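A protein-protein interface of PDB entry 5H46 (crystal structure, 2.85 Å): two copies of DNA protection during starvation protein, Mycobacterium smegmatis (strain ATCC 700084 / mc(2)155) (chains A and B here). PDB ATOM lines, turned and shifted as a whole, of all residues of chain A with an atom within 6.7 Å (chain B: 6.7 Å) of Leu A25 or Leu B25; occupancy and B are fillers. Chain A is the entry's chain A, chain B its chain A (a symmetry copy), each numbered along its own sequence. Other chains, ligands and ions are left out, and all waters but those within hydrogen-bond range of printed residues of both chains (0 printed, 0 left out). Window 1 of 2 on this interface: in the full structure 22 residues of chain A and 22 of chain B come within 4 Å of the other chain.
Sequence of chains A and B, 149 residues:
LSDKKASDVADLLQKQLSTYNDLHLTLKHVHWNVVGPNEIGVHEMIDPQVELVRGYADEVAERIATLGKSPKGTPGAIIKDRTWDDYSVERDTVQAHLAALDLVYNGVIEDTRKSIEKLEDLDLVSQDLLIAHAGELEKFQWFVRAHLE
Tyr A20 touches none of the printed residues of chain B. Of the printed residues of chain B, Asn A21 touches Trp B32. Of the printed residues of chain B, Asp A22 touches Pro B75. Of the printed residues of chain B, Leu A25 touches Leu B25 (3.3 Å), Gly B73 (3.8 Å) and Pro B75 (3.996 Å). Printed residues of chain B within 4 Å of Trp A32: Asn B21. Ile A78 touches none of the printed residues of chain B. Printed residues of chain A within 4 Å of Asn B21: Trp A32. Of the printed residues of chain A, Leu B25 touches Leu A25 (3.3 Å), Gly A73 (3.8 Å) and Pro A75 (3.99 Å). Of the printed residues of chain A, Gly B73 touches Leu A25 and His A29. The nearest printed residue of chain A that does not touch Leu B25 is Asn A21 (4.2 Å). The nearest printed residue of chain A that does not touch His B29 is Pro A75 (7.1 Å).
Hydrophobic or aromatic side chains of chain B within 4 Å of the printed part of chain A: Leu B25, His B29, Trp B32 and Pro B75. Among the printed residues, 13 pairs touch across the chains.
A ring nitrogen (NE2) of His A24 is in hydrogen-bond range of the side-chain amide oxygen (OD1) of Asn A21, 3.2 Å away. O of Asp A22 is in hydrogen-bond range of OG1 of Thr A26, at 2.7 Å. The side-chain amide oxygen of Asn B21 is in hydrogen-bond range of a ring nitrogen (NE2) of His B24 (3.2 Å). O of Asp B22 sits at hydrogen-bond distance from OG1 of Thr B26 (2.7 Å).
Asn A21 touches Trp B32, and with the chains exchanged Trp A32 touches Asn B21. Leu A25 touches Pro B75, and with the chains exchanged Pro A75 touches Leu B25. His A29 touches Gly B73, and with the chains exchanged Gly A73 touches His B29. His A29 touches Thr B74, and with the chains exchanged Thr A74 touches His B29. Positions printed for both chains: 20, 21, 22, 23, 24, 25, 26, 27, 28, 29, 30, 32, 53, 73, 74, 75 and 78.
OD1 of Asp A22 touches CG of Pro B75, 3.0 Å away. Leu A25 touches Leu B25. Gly B73 touches Leu A25. CG of Pro B75 touches CD1 of Leu A25, at 3.996 Å. Gly B73 touches His A29 (N to CD2, 3.3 Å). His A29 touches Thr B74 (CG to CG2, 3.7 Å). Trp A32 touches Asn B21 (CH2 to OD1, 3.9 Å). Gly A73 touches Leu B25 (O to CB, 3.8 Å). Thr A74 touches His B29. Pro A75 touches Leu B25.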
ATOM      1  N   TYR A  20      -7.273  26.406  -8.909  1.00  0.00           N
ATOM      2  CA  TYR A  20      -6.824  25.332  -9.776  1.00  0.00           C
ATOM      3  C   TYR A  20      -5.542  24.726  -9.269  1.00  0.00           C
ATOM      4  O   TYR A  20      -5.432  23.501  -9.141  1.00  0.00           O
ATOM      5  CB  TYR A  20      -6.683  25.818 -11.229  1.00  0.00           C
ATOM      6  CG  TYR A  20      -7.985  26.173 -11.945  1.00  0.00           C
ATOM      7  CD1 TYR A  20      -8.004  27.182 -12.924  1.00  0.00           C
ATOM      8  CD2 TYR A  20      -9.174  25.542 -11.629  1.00  0.00           C
ATOM      9  CE1 TYR A  20      -9.175  27.532 -13.553  1.00  0.00           C
ATOM     10  CE2 TYR A  20     -10.359  25.866 -12.266  1.00  0.00           C
ATOM     11  CZ  TYR A  20     -10.343  26.861 -13.232  1.00  0.00           C
ATOM     12  OH  TYR A  20     -11.535  27.161 -13.860  1.00  0.00           O
ATOM     13  N   ASN A  21      -4.567  25.564  -8.985  1.00  0.00           N
ATOM     14  CA  ASN A  21      -3.312  25.044  -8.435  1.00  0.00           C
ATOM     15  C   ASN A  21      -3.556  24.229  -7.179  1.00  0.00           C
ATOM     16  O   ASN A  21      -2.922  23.200  -6.982  1.00  0.00           O
ATOM     17  CB  ASN A  21      -2.337  26.161  -8.156  1.00  0.00           C
ATOM     18  CG  ASN A  21      -1.800  26.801  -9.417  1.00  0.00           C
ATOM     19  OD1 ASN A  21      -1.409  26.117 -10.368  1.00  0.00           O
ATOM     20  ND2 ASN A  21      -1.740  28.134  -9.416  1.00  0.00           N
ATOM     21  N   ASP A  22      -4.494  24.689  -6.348  1.00  0.00           N
ATOM     22  CA  ASP A  22      -4.863  23.979  -5.143  1.00  0.00           C
ATOM     23  C   ASP A  22      -5.454  22.615  -5.522  1.00  0.00           C
ATOM     24  O   ASP A  22      -5.144  21.584  -4.904  1.00  0.00           O
ATOM     25  CB  ASP A  22      -5.845  24.814  -4.296  1.00  0.00           C
ATOM     26  CG  ASP A  22      -6.309  24.064  -3.020  1.00  0.00           C
ATOM     27  OD1 ASP A  22      -5.583  24.022  -2.013  1.00  0.00           O
ATOM     28  OD2 ASP A  22      -7.418  23.497  -3.012  1.00  0.00           O
ATOM     29  N   LEU A  23      -6.317  22.619  -6.522  1.00  0.00           N
ATOM     30  CA  LEU A  23      -6.972  21.388  -6.939  1.00  0.00           C
ATOM     31  C   LEU A  23      -5.970  20.354  -7.527  1.00  0.00           C
ATOM     32  O   LEU A  23      -5.996  19.171  -7.192  1.00  0.00           O
ATOM     33  CB  LEU A  23      -8.071  21.699  -7.962  1.00  0.00           C
ATOM     34  CG  LEU A  23      -8.706  20.474  -8.560  1.00  0.00           C
ATOM     35  CD1 LEU A  23      -9.277  19.531  -7.538  1.00  0.00           C
ATOM     36  CD2 LEU A  23      -9.807  20.928  -9.486  1.00  0.00           C
ATOM     37  N   HIS A  24      -5.086  20.791  -8.405  1.00  0.00           N
ATOM     38  CA  HIS A  24      -4.231  19.828  -9.003  1.00  0.00           C
ATOM     39  C   HIS A  24      -3.049  19.413  -8.146  1.00  0.00           C
ATOM     40  O   HIS A  24      -2.393  18.416  -8.460  1.00  0.00           O
ATOM     41  CB  HIS A  24      -3.833  20.278 -10.404  1.00  0.00           C
ATOM     42  CG  HIS A  24      -2.694  21.242 -10.459  1.00  0.00           C
ATOM     43  ND1 HIS A  24      -1.380  20.853 -10.270  1.00  0.00           N
ATOM     44  CD2 HIS A  24      -2.675  22.551 -10.808  1.00  0.00           C
ATOM     45  CE1 HIS A  24      -0.604  21.910 -10.432  1.00  0.00           C
ATOM     46  NE2 HIS A  24      -1.366  22.951 -10.759  1.00  0.00           N
ATOM     47  N   LEU A  25      -2.764  20.149  -7.067  1.00  0.00           N
ATOM     48  CA  LEU A  25      -1.901  19.614  -6.014  1.00  0.00           C
ATOM     49  C   LEU A  25      -2.647  18.580  -5.202  1.00  0.00           C
ATOM     50  O   LEU A  25      -2.080  17.545  -4.828  1.00  0.00           O
ATOM     51  CB  LEU A  25      -1.384  20.710  -5.138  1.00  0.00           C
ATOM     52  CG  LEU A  25      -0.389  21.664  -5.770  1.00  0.00           C
ATOM     53  CD1 LEU A  25      -0.206  22.868  -4.863  1.00  0.00           C
ATOM     54  CD2 LEU A  25       0.928  20.938  -5.937  1.00  0.00           C
ATOM     55  N   THR A  26      -3.908  18.881  -4.916  1.00  0.00           N
ATOM     56  CA  THR A  26      -4.779  17.944  -4.208  1.00  0.00           C
ATOM     57  C   THR A  26      -5.012  16.672  -5.015  1.00  0.00           C
ATOM     58  O   THR A  26      -4.965  15.577  -4.451  1.00  0.00           O
ATOM     59  CB  THR A  26      -6.139  18.608  -3.883  1.00  0.00           C
ATOM     60  OG1 THR A  26      -5.901  19.729  -3.043  1.00  0.00           O
ATOM     61  CG2 THR A  26      -7.113  17.631  -3.203  1.00  0.00           C
ATOM     62  N   LEU A  27      -5.243  16.833  -6.325  1.00  0.00           N
ATOM     63  CA  LEU A  27      -5.429  15.686  -7.219  1.00  0.00           C
ATOM     64  C   LEU A  27      -4.212  14.827  -7.200  1.00  0.00           C
ATOM     65  O   LEU A  27      -4.308  13.604  -7.061  1.00  0.00           O
ATOM     66  CB  LEU A  27      -5.772  16.125  -8.645  1.00  0.00           C
ATOM     67  CG  LEU A  27      -7.255  16.358  -8.805  1.00  0.00           C
ATOM     68  CD1 LEU A  27      -7.611  17.100 -10.092  1.00  0.00           C
ATOM     69  CD2 LEU A  27      -7.995  15.041  -8.670  1.00  0.00           C
ATOM     70  N   LYS A  28      -3.044  15.454  -7.312  1.00  0.00           N
ATOM     71  CA  LYS A  28      -1.784  14.700  -7.252  1.00  0.00           C
ATOM     72  C   LYS A  28      -1.568  14.091  -5.894  1.00  0.00           C
ATOM     73  O   LYS A  28      -0.889  13.095  -5.785  1.00  0.00           O
ATOM     74  CB  LYS A  28      -0.612  15.574  -7.692  1.00  0.00           C
ATOM     75  CG  LYS A  28       0.576  14.800  -8.217  1.00  0.00           C
ATOM     76  CD  LYS A  28       0.354  14.221  -9.626  1.00  0.00           C
ATOM     77  CE  LYS A  28       1.572  13.428 -10.136  1.00  0.00           C
ATOM     78  NZ  LYS A  28       2.613  14.270 -10.900  1.00  0.00           N
ATOM     79  N   HIS A  29      -2.156  14.672  -4.861  1.00  0.00           N
ATOM     80  CA  HIS A  29      -2.064  14.103  -3.496  1.00  0.00           C
ATOM     81  C   HIS A  29      -2.934  12.882  -3.339  1.00  0.00           C
ATOM     82  O   HIS A  29      -2.447  11.854  -2.864  1.00  0.00           O
ATOM     83  CB  HIS A  29      -2.397  15.171  -2.422  1.00  0.00           C
ATOM     84  CG  HIS A  29      -2.556  14.605  -1.037  1.00  0.00           C
ATOM     85  ND1 HIS A  29      -3.772  14.220  -0.511  1.00  0.00           N
ATOM     86  CD2 HIS A  29      -1.639  14.356  -0.082  1.00  0.00           C
ATOM     87  CE1 HIS A  29      -3.586  13.718   0.694  1.00  0.00           C
ATOM     88  NE2 HIS A  29      -2.294  13.775   0.965  1.00  0.00           N
ATOM     89  N   VAL A  30      -4.189  12.981  -3.750  1.00  0.00           N
ATOM     90  CA  VAL A  30      -5.079  11.811  -3.687  1.00  0.00           C
ATOM     91  C   VAL A  30      -4.521  10.701  -4.562  1.00  0.00           C
ATOM     92  O   VAL A  30      -4.574   9.531  -4.171  1.00  0.00           O
ATOM     93  CB  VAL A  30      -6.566  12.135  -4.011  1.00  0.00           C
ATOM     94  CG1 VAL A  30      -7.024  13.358  -3.243  1.00  0.00           C
ATOM     95  CG2 VAL A  30      -6.761  12.421  -5.436  1.00  0.00           C
ATOM     96  N   TRP A  32      -1.385   9.962  -5.176  1.00  0.00           N
ATOM     97  CA  TRP A  32      -0.283   9.281  -4.491  1.00  0.00           C
ATOM     98  C   TRP A  32      -0.679   8.328  -3.383  1.00  0.00           C
ATOM     99  O   TRP A  32       0.132   7.480  -3.037  1.00  0.00           O
ATOM    100  CB  TRP A  32       0.686  10.295  -3.896  1.00  0.00           C
ATOM    101  CG  TRP A  32       1.516  11.050  -4.898  1.00  0.00           C
ATOM    102  CD1 TRP A  32       2.065  10.551  -6.022  1.00  0.00           C
ATOM    103  CD2 TRP A  32       1.950  12.418  -4.816  1.00  0.00           C
ATOM    104  NE1 TRP A  32       2.772  11.511  -6.683  1.00  0.00           N
ATOM    105  CE2 TRP A  32       2.729  12.674  -5.953  1.00  0.00           C
ATOM    106  CE3 TRP A  32       1.727  13.458  -3.909  1.00  0.00           C
ATOM    107  CZ2 TRP A  32       3.300  13.921  -6.207  1.00  0.00           C
ATOM    108  CZ3 TRP A  32       2.285  14.702  -4.182  1.00  0.00           C
ATOM    109  CH2 TRP A  32       3.049  14.913  -5.339  1.00  0.00           C
ATOM    110  N   VAL A  53      -6.778  19.987 -15.361  1.00  0.00           N
ATOM    111  CA  VAL A  53      -6.786  21.121 -14.433  1.00  0.00           C
ATOM    112  C   VAL A  53      -5.559  22.029 -14.625  1.00  0.00           C
ATOM    113  O   VAL A  53      -5.703  23.253 -14.762  1.00  0.00           O
ATOM    114  CB  VAL A  53      -6.901  20.643 -12.981  1.00  0.00           C
ATOM    115  CG1 VAL A  53      -6.767  21.811 -12.014  1.00  0.00           C
ATOM    116  CG2 VAL A  53      -8.266  19.983 -12.763  1.00  0.00           C
ATOM    117  N   GLY A  73       0.988  32.082  -8.849  1.00  0.00           N
ATOM    118  CA  GLY A  73       0.598  30.726  -8.463  1.00  0.00           C
ATOM    119  C   GLY A  73       1.561  30.123  -7.501  1.00  0.00           C
ATOM    120  O   GLY A  73       1.642  28.918  -7.360  1.00  0.00           O
ATOM    121  N   THR A  74       2.207  31.000  -6.740  1.00  0.00           N
ATOM    122  CA  THR A  74       3.104  30.624  -5.645  1.00  0.00           C
ATOM    123  C   THR A  74       2.294  30.022  -4.475  1.00  0.00           C
ATOM    124  O   THR A  74       1.111  30.316  -4.318  1.00  0.00           O
ATOM    125  CB  THR A  74       3.883  31.832  -5.147  1.00  0.00           C
ATOM    126  OG1 THR A  74       2.973  32.865  -4.725  1.00  0.00           O
ATOM    127  CG2 THR A  74       4.742  32.396  -6.224  1.00  0.00           C
ATOM    128  N   PRO A  75       2.932  29.187  -3.651  1.00  0.00           N
ATOM    129  CA  PRO A  75       2.126  28.495  -2.617  1.00  0.00           C
ATOM    130  C   PRO A  75       1.480  29.426  -1.598  1.00  0.00           C
ATOM    131  O   PRO A  75       0.358  29.154  -1.157  1.00  0.00           O
ATOM    132  CB  PRO A  75       3.137  27.535  -1.955  1.00  0.00           C
ATOM    133  CG  PRO A  75       4.163  27.310  -3.010  1.00  0.00           C
ATOM    134  CD  PRO A  75       4.319  28.668  -3.693  1.00  0.00           C
ATOM    135  N   ILE A  78      -1.815  30.580  -2.740  1.00  0.00           N
ATOM    136  CA  ILE A  78      -2.853  29.556  -2.795  1.00  0.00           C
ATOM    137  C   ILE A  78      -3.613  29.560  -1.467  1.00  0.00           C
ATOM    138  O   ILE A  78      -4.817  29.670  -1.446  1.00  0.00           O
ATOM    139  CB  ILE A  78      -2.247  28.144  -3.095  1.00  0.00           C
ATOM    140  CG1 ILE A  78      -1.133  28.204  -4.156  1.00  0.00           C
ATOM    141  CG2 ILE A  78      -3.304  27.170  -3.559  1.00  0.00           C
ATOM    142  CD1 ILE A  78      -1.556  28.614  -5.550  1.00  0.00           C
ATOM    143  N   TYR B  20       9.729  20.225  -3.395  1.00  0.00           N
ATOM    144  CA  TYR B  20       9.572  20.051  -4.828  1.00  0.00           C
ATOM    145  C   TYR B  20       8.287  20.670  -5.311  1.00  0.00           C
ATOM    146  O   TYR B  20       8.284  21.439  -6.279  1.00  0.00           O
ATOM    147  CB  TYR B  20       9.665  18.566  -5.216  1.00  0.00           C
ATOM    148  CG  TYR B  20      11.036  17.914  -5.046  1.00  0.00           C
ATOM    149  CD1 TYR B  20      11.139  16.549  -4.722  1.00  0.00           C
ATOM    150  CD2 TYR B  20      12.201  18.648  -5.172  1.00  0.00           C
ATOM    151  CE1 TYR B  20      12.366  15.959  -4.536  1.00  0.00           C
ATOM    152  CE2 TYR B  20      13.446  18.067  -5.010  1.00  0.00           C
ATOM    153  CZ  TYR B  20      13.513  16.718  -4.697  1.00  0.00           C
ATOM    154  OH  TYR B  20      14.767  16.157  -4.547  1.00  0.00           O
ATOM    155  N   ASN B  21       7.193  20.341  -4.657  1.00  0.00           N
ATOM    156  CA  ASN B  21       5.917  20.951  -5.041  1.00  0.00           C
ATOM    157  C   ASN B  21       5.997  22.465  -5.008  1.00  0.00           C
ATOM    158  O   ASN B  21       5.449  23.128  -5.880  1.00  0.00           O
ATOM    159  CB  ASN B  21       4.794  20.464  -4.158  1.00  0.00           C
ATOM    160  CG  ASN B  21       4.448  19.011  -4.396  1.00  0.00           C
ATOM    161  OD1 ASN B  21       4.322  18.559  -5.538  1.00  0.00           O
ATOM    162  ND2 ASN B  21       4.248  18.272  -3.303  1.00  0.00           N
ATOM    163  N   ASP B  22       6.703  22.999  -4.008  1.00  0.00           N
ATOM    164  CA  ASP B  22       6.904  24.426  -3.891  1.00  0.00           C
ATOM    165  C   ASP B  22       7.697  24.925  -5.105  1.00  0.00           C
ATOM    166  O   ASP B  22       7.383  25.973  -5.694  1.00  0.00           O
ATOM    167  CB  ASP B  22       7.609  24.771  -2.564  1.00  0.00           C
ATOM    168  CG  ASP B  22       7.893  26.290  -2.424  1.00  0.00           C
ATOM    169  OD1 ASP B  22       6.995  27.071  -2.070  1.00  0.00           O
ATOM    170  OD2 ASP B  22       9.033  26.725  -2.673  1.00  0.00           O
ATOM    171  N   LEU B  23       8.732  24.186  -5.460  1.00  0.00           N
ATOM    172  CA  LEU B  23       9.581  24.588  -6.572  1.00  0.00           C
ATOM    173  C   LEU B  23       8.826  24.565  -7.932  1.00  0.00           C
ATOM    174  O   LEU B  23       8.912  25.497  -8.731  1.00  0.00           O
ATOM    175  CB  LEU B  23      10.819  23.685  -6.640  1.00  0.00           C
ATOM    176  CG  LEU B  23      11.683  23.932  -7.846  1.00  0.00           C
ATOM    177  CD1 LEU B  23      12.141  25.357  -7.979  1.00  0.00           C
ATOM    178  CD2 LEU B  23      12.889  23.030  -7.743  1.00  0.00           C
ATOM    179  N   HIS B  24       8.089  23.504  -8.203  1.00  0.00           N
ATOM    180  CA  HIS B  24       7.472  23.449  -9.481  1.00  0.00           C
ATOM    181  C   HIS B  24       6.197  24.263  -9.603  1.00  0.00           C
ATOM    182  O   HIS B  24       5.722  24.483 -10.722  1.00  0.00           O
ATOM    183  CB  HIS B  24       7.309  22.000  -9.923  1.00  0.00           C
ATOM    184  CG  HIS B  24       6.106  21.303  -9.374  1.00  0.00           C
ATOM    185  ND1 HIS B  24       4.829  21.535  -9.852  1.00  0.00           N
ATOM    186  CD2 HIS B  24       6.018  20.292  -8.477  1.00  0.00           C
ATOM    187  CE1 HIS B  24       3.992  20.738  -9.212  1.00  0.00           C
ATOM    188  NE2 HIS B  24       4.689  19.974  -8.374  1.00  0.00           N
ATOM    189  N   LEU B  25       5.632  24.721  -8.482  1.00  0.00           N
ATOM    190  CA  LEU B  25       4.643  25.797  -8.537  1.00  0.00           C
ATOM    191  C   LEU B  25       5.321  27.118  -8.823  1.00  0.00           C
ATOM    192  O   LEU B  25       4.805  27.937  -9.593  1.00  0.00           O
ATOM    193  CB  LEU B  25       3.853  25.864  -7.270  1.00  0.00           C
ATOM    194  CG  LEU B  25       2.905  24.712  -7.005  1.00  0.00           C
ATOM    195  CD1 LEU B  25       2.424  24.781  -5.566  1.00  0.00           C
ATOM    196  CD2 LEU B  25       1.729  24.835  -7.950  1.00  0.00           C
ATOM    197  N   THR B  26       6.464  27.321  -8.178  1.00  0.00           N
ATOM    198  CA  THR B  26       7.275  28.515  -8.413  1.00  0.00           C
ATOM    199  C   THR B  26       7.793  28.572  -9.846  1.00  0.00           C
ATOM    200  O   THR B  26       7.753  29.637 -10.465  1.00  0.00           O
ATOM    201  CB  THR B  26       8.469  28.562  -7.429  1.00  0.00           C
ATOM    202  OG1 THR B  26       7.956  28.615  -6.105  1.00  0.00           O
ATOM    203  CG2 THR B  26       9.390  29.765  -7.691  1.00  0.00           C
ATOM    204  N   LEU B  27       8.256  27.422 -10.357  1.00  0.00           N
ATOM    205  CA  LEU B  27       8.731  27.333 -11.741  1.00  0.00           C
ATOM    206  C   LEU B  27       7.630  27.694 -12.678  1.00  0.00           C
ATOM    207  O   LEU B  27       7.826  28.492 -13.599  1.00  0.00           O
ATOM    208  CB  LEU B  27       9.295  25.947 -12.061  1.00  0.00           C
ATOM    209  CG  LEU B  27      10.748  25.842 -11.664  1.00  0.00           C
ATOM    210  CD1 LEU B  27      11.267  24.405 -11.657  1.00  0.00           C
ATOM    211  CD2 LEU B  27      11.583  26.757 -12.540  1.00  0.00           C
ATOM    212  N   LYS B  28       6.447  27.134 -12.444  1.00  0.00           N
ATOM    213  CA  LYS B  28       5.286  27.466 -13.281  1.00  0.00           C
ATOM    214  C   LYS B  28       4.876  28.903 -13.113  1.00  0.00           C
ATOM    215  O   LYS B  28       4.297  29.470 -14.012  1.00  0.00           O
ATOM    216  CB  LYS B  28       4.136  26.497 -13.016  1.00  0.00           C
ATOM    217  CG  LYS B  28       3.161  26.363 -14.163  1.00  0.00           C
ATOM    218  CD  LYS B  28       3.711  25.538 -15.341  1.00  0.00           C
ATOM    219  CE  LYS B  28       2.706  25.424 -16.502  1.00  0.00           C
ATOM    220  NZ  LYS B  28       1.749  24.218 -16.408  1.00  0.00           N
ATOM    221  N   HIS B  29       5.187  29.500 -11.974  1.00  0.00           N
ATOM    222  CA  HIS B  29       4.893  30.934 -11.746  1.00  0.00           C
ATOM    223  C   HIS B  29       5.840  31.828 -12.505  1.00  0.00           C
ATOM    224  O   HIS B  29       5.381  32.736 -13.201  1.00  0.00           O
ATOM    225  CB  HIS B  29       4.897  31.270 -10.232  1.00  0.00           C
ATOM    226  CG  HIS B  29       4.844  32.746  -9.941  1.00  0.00           C
ATOM    227  ND1 HIS B  29       5.968  33.521  -9.748  1.00  0.00           N
ATOM    228  CD2 HIS B  29       3.790  33.577  -9.822  1.00  0.00           C
ATOM    229  CE1 HIS B  29       5.606  34.776  -9.565  1.00  0.00           C
ATOM    230  NE2 HIS B  29       4.288  34.833  -9.626  1.00  0.00           N
ATOM    231  N   VAL B  30       7.133  31.565 -12.396  1.00  0.00           N
ATOM    232  CA  VAL B  30       8.112  32.355 -13.160  1.00  0.00           C
ATOM    233  C   VAL B  30       7.855  32.183 -14.647  1.00  0.00           C
ATOM    234  O   VAL B  30       7.953  33.157 -15.400  1.00  0.00           O
ATOM    235  CB  VAL B  30       9.591  32.065 -12.774  1.00  0.00           C
ATOM    236  CG1 VAL B  30       9.760  32.075 -11.268  1.00  0.00           C
ATOM    237  CG2 VAL B  30      10.028  30.748 -13.248  1.00  0.00           C
ATOM    238  N   TRP B  32       4.993  31.751 -16.190  1.00  0.00           N
ATOM    239  CA  TRP B  32       3.857  32.578 -16.607  1.00  0.00           C
ATOM    240  C   TRP B  32       4.128  34.062 -16.737  1.00  0.00           C
ATOM    241  O   TRP B  32       3.359  34.730 -17.414  1.00  0.00           O
ATOM    242  CB  TRP B  32       2.689  32.410 -15.642  1.00  0.00           C
ATOM    243  CG  TRP B  32       1.994  31.077 -15.706  1.00  0.00           C
ATOM    244  CD1 TRP B  32       1.729  30.364 -16.817  1.00  0.00           C
ATOM    245  CD2 TRP B  32       1.411  30.346 -14.613  1.00  0.00           C
ATOM    246  NE1 TRP B  32       1.067  29.213 -16.505  1.00  0.00           N
ATOM    247  CE2 TRP B  32       0.845  29.182 -15.150  1.00  0.00           C
ATOM    248  CE3 TRP B  32       1.344  30.549 -13.232  1.00  0.00           C
ATOM    249  CZ2 TRP B  32       0.206  28.225 -14.362  1.00  0.00           C
ATOM    250  CZ3 TRP B  32       0.721  29.578 -12.453  1.00  0.00           C
ATOM    251  CH2 TRP B  32       0.179  28.424 -13.036  1.00  0.00           C
ATOM    252  N   VAL B  53      11.172  18.365 -12.200  1.00  0.00           N
ATOM    253  CA  VAL B  53      10.881  18.510 -10.771  1.00  0.00           C
ATOM    254  C   VAL B  53       9.626  17.721 -10.358  1.00  0.00           C
ATOM    255  O   VAL B  53       9.664  16.949  -9.389  1.00  0.00           O
ATOM    256  CB  VAL B  53      10.761  19.988 -10.381  1.00  0.00           C
ATOM    257  CG1 VAL B  53      10.321  20.131  -8.931  1.00  0.00           C
ATOM    258  CG2 VAL B  53      12.120  20.675 -10.549  1.00  0.00           C
ATOM    259  N   GLY B  73       1.062  16.281  -0.265  1.00  0.00           N
ATOM    260  CA  GLY B  73       1.511  17.388  -1.109  1.00  0.00           C
ATOM    261  C   GLY B  73       0.448  18.415  -1.289  1.00  0.00           C
ATOM    262  O   GLY B  73       0.469  19.187  -2.229  1.00  0.00           O
ATOM    263  N   THR B  74      -0.421  18.495  -0.287  1.00  0.00           N
ATOM    264  CA  THR B  74      -1.469  19.514  -0.196  1.00  0.00           C
ATOM    265  C   THR B  74      -0.842  20.900   0.078  1.00  0.00           C
ATOM    266  O   THR B  74       0.250  20.992   0.632  1.00  0.00           O
ATOM    267  CB  THR B  74      -2.452  19.179   0.914  1.00  0.00           C
ATOM    268  OG1 THR B  74      -1.756  19.055   2.168  1.00  0.00           O
ATOM    269  CG2 THR B  74      -3.141  17.886   0.649  1.00  0.00           C
ATOM    270  N   PRO B  75      -1.536  21.974  -0.305  1.00  0.00           N
ATOM    271  CA  PRO B  75      -0.878  23.296  -0.178  1.00  0.00           C
ATOM    272  C   PRO B  75      -0.544  23.695   1.255  1.00  0.00           C
ATOM    273  O   PRO B  75       0.493  24.328   1.479  1.00  0.00           O
ATOM    274  CB  PRO B  75      -1.892  24.267  -0.821  1.00  0.00           C
ATOM    275  CG  PRO B  75      -2.664  23.410  -1.760  1.00  0.00           C
ATOM    276  CD  PRO B  75      -2.826  22.079  -1.026  1.00  0.00           C
ATOM    277  N   ILE B  78       2.770  22.461   2.248  1.00  0.00           N
ATOM    278  CA  ILE B  78       3.901  23.089   1.573  1.00  0.00           C
ATOM    279  C   ILE B  78       4.384  24.266   2.422  1.00  0.00           C
ATOM    280  O   ILE B  78       5.543  24.349   2.758  1.00  0.00           O
ATOM    281  CB  ILE B  78       3.517  23.554   0.128  1.00  0.00           C
ATOM    282  CG1 ILE B  78       2.629  22.525  -0.596  1.00  0.00           C
ATOM    283  CG2 ILE B  78       4.740  23.817  -0.718  1.00  0.00           C
ATOM    284  CD1 ILE B  78       3.269  21.190  -0.908  1.00  0.00           C
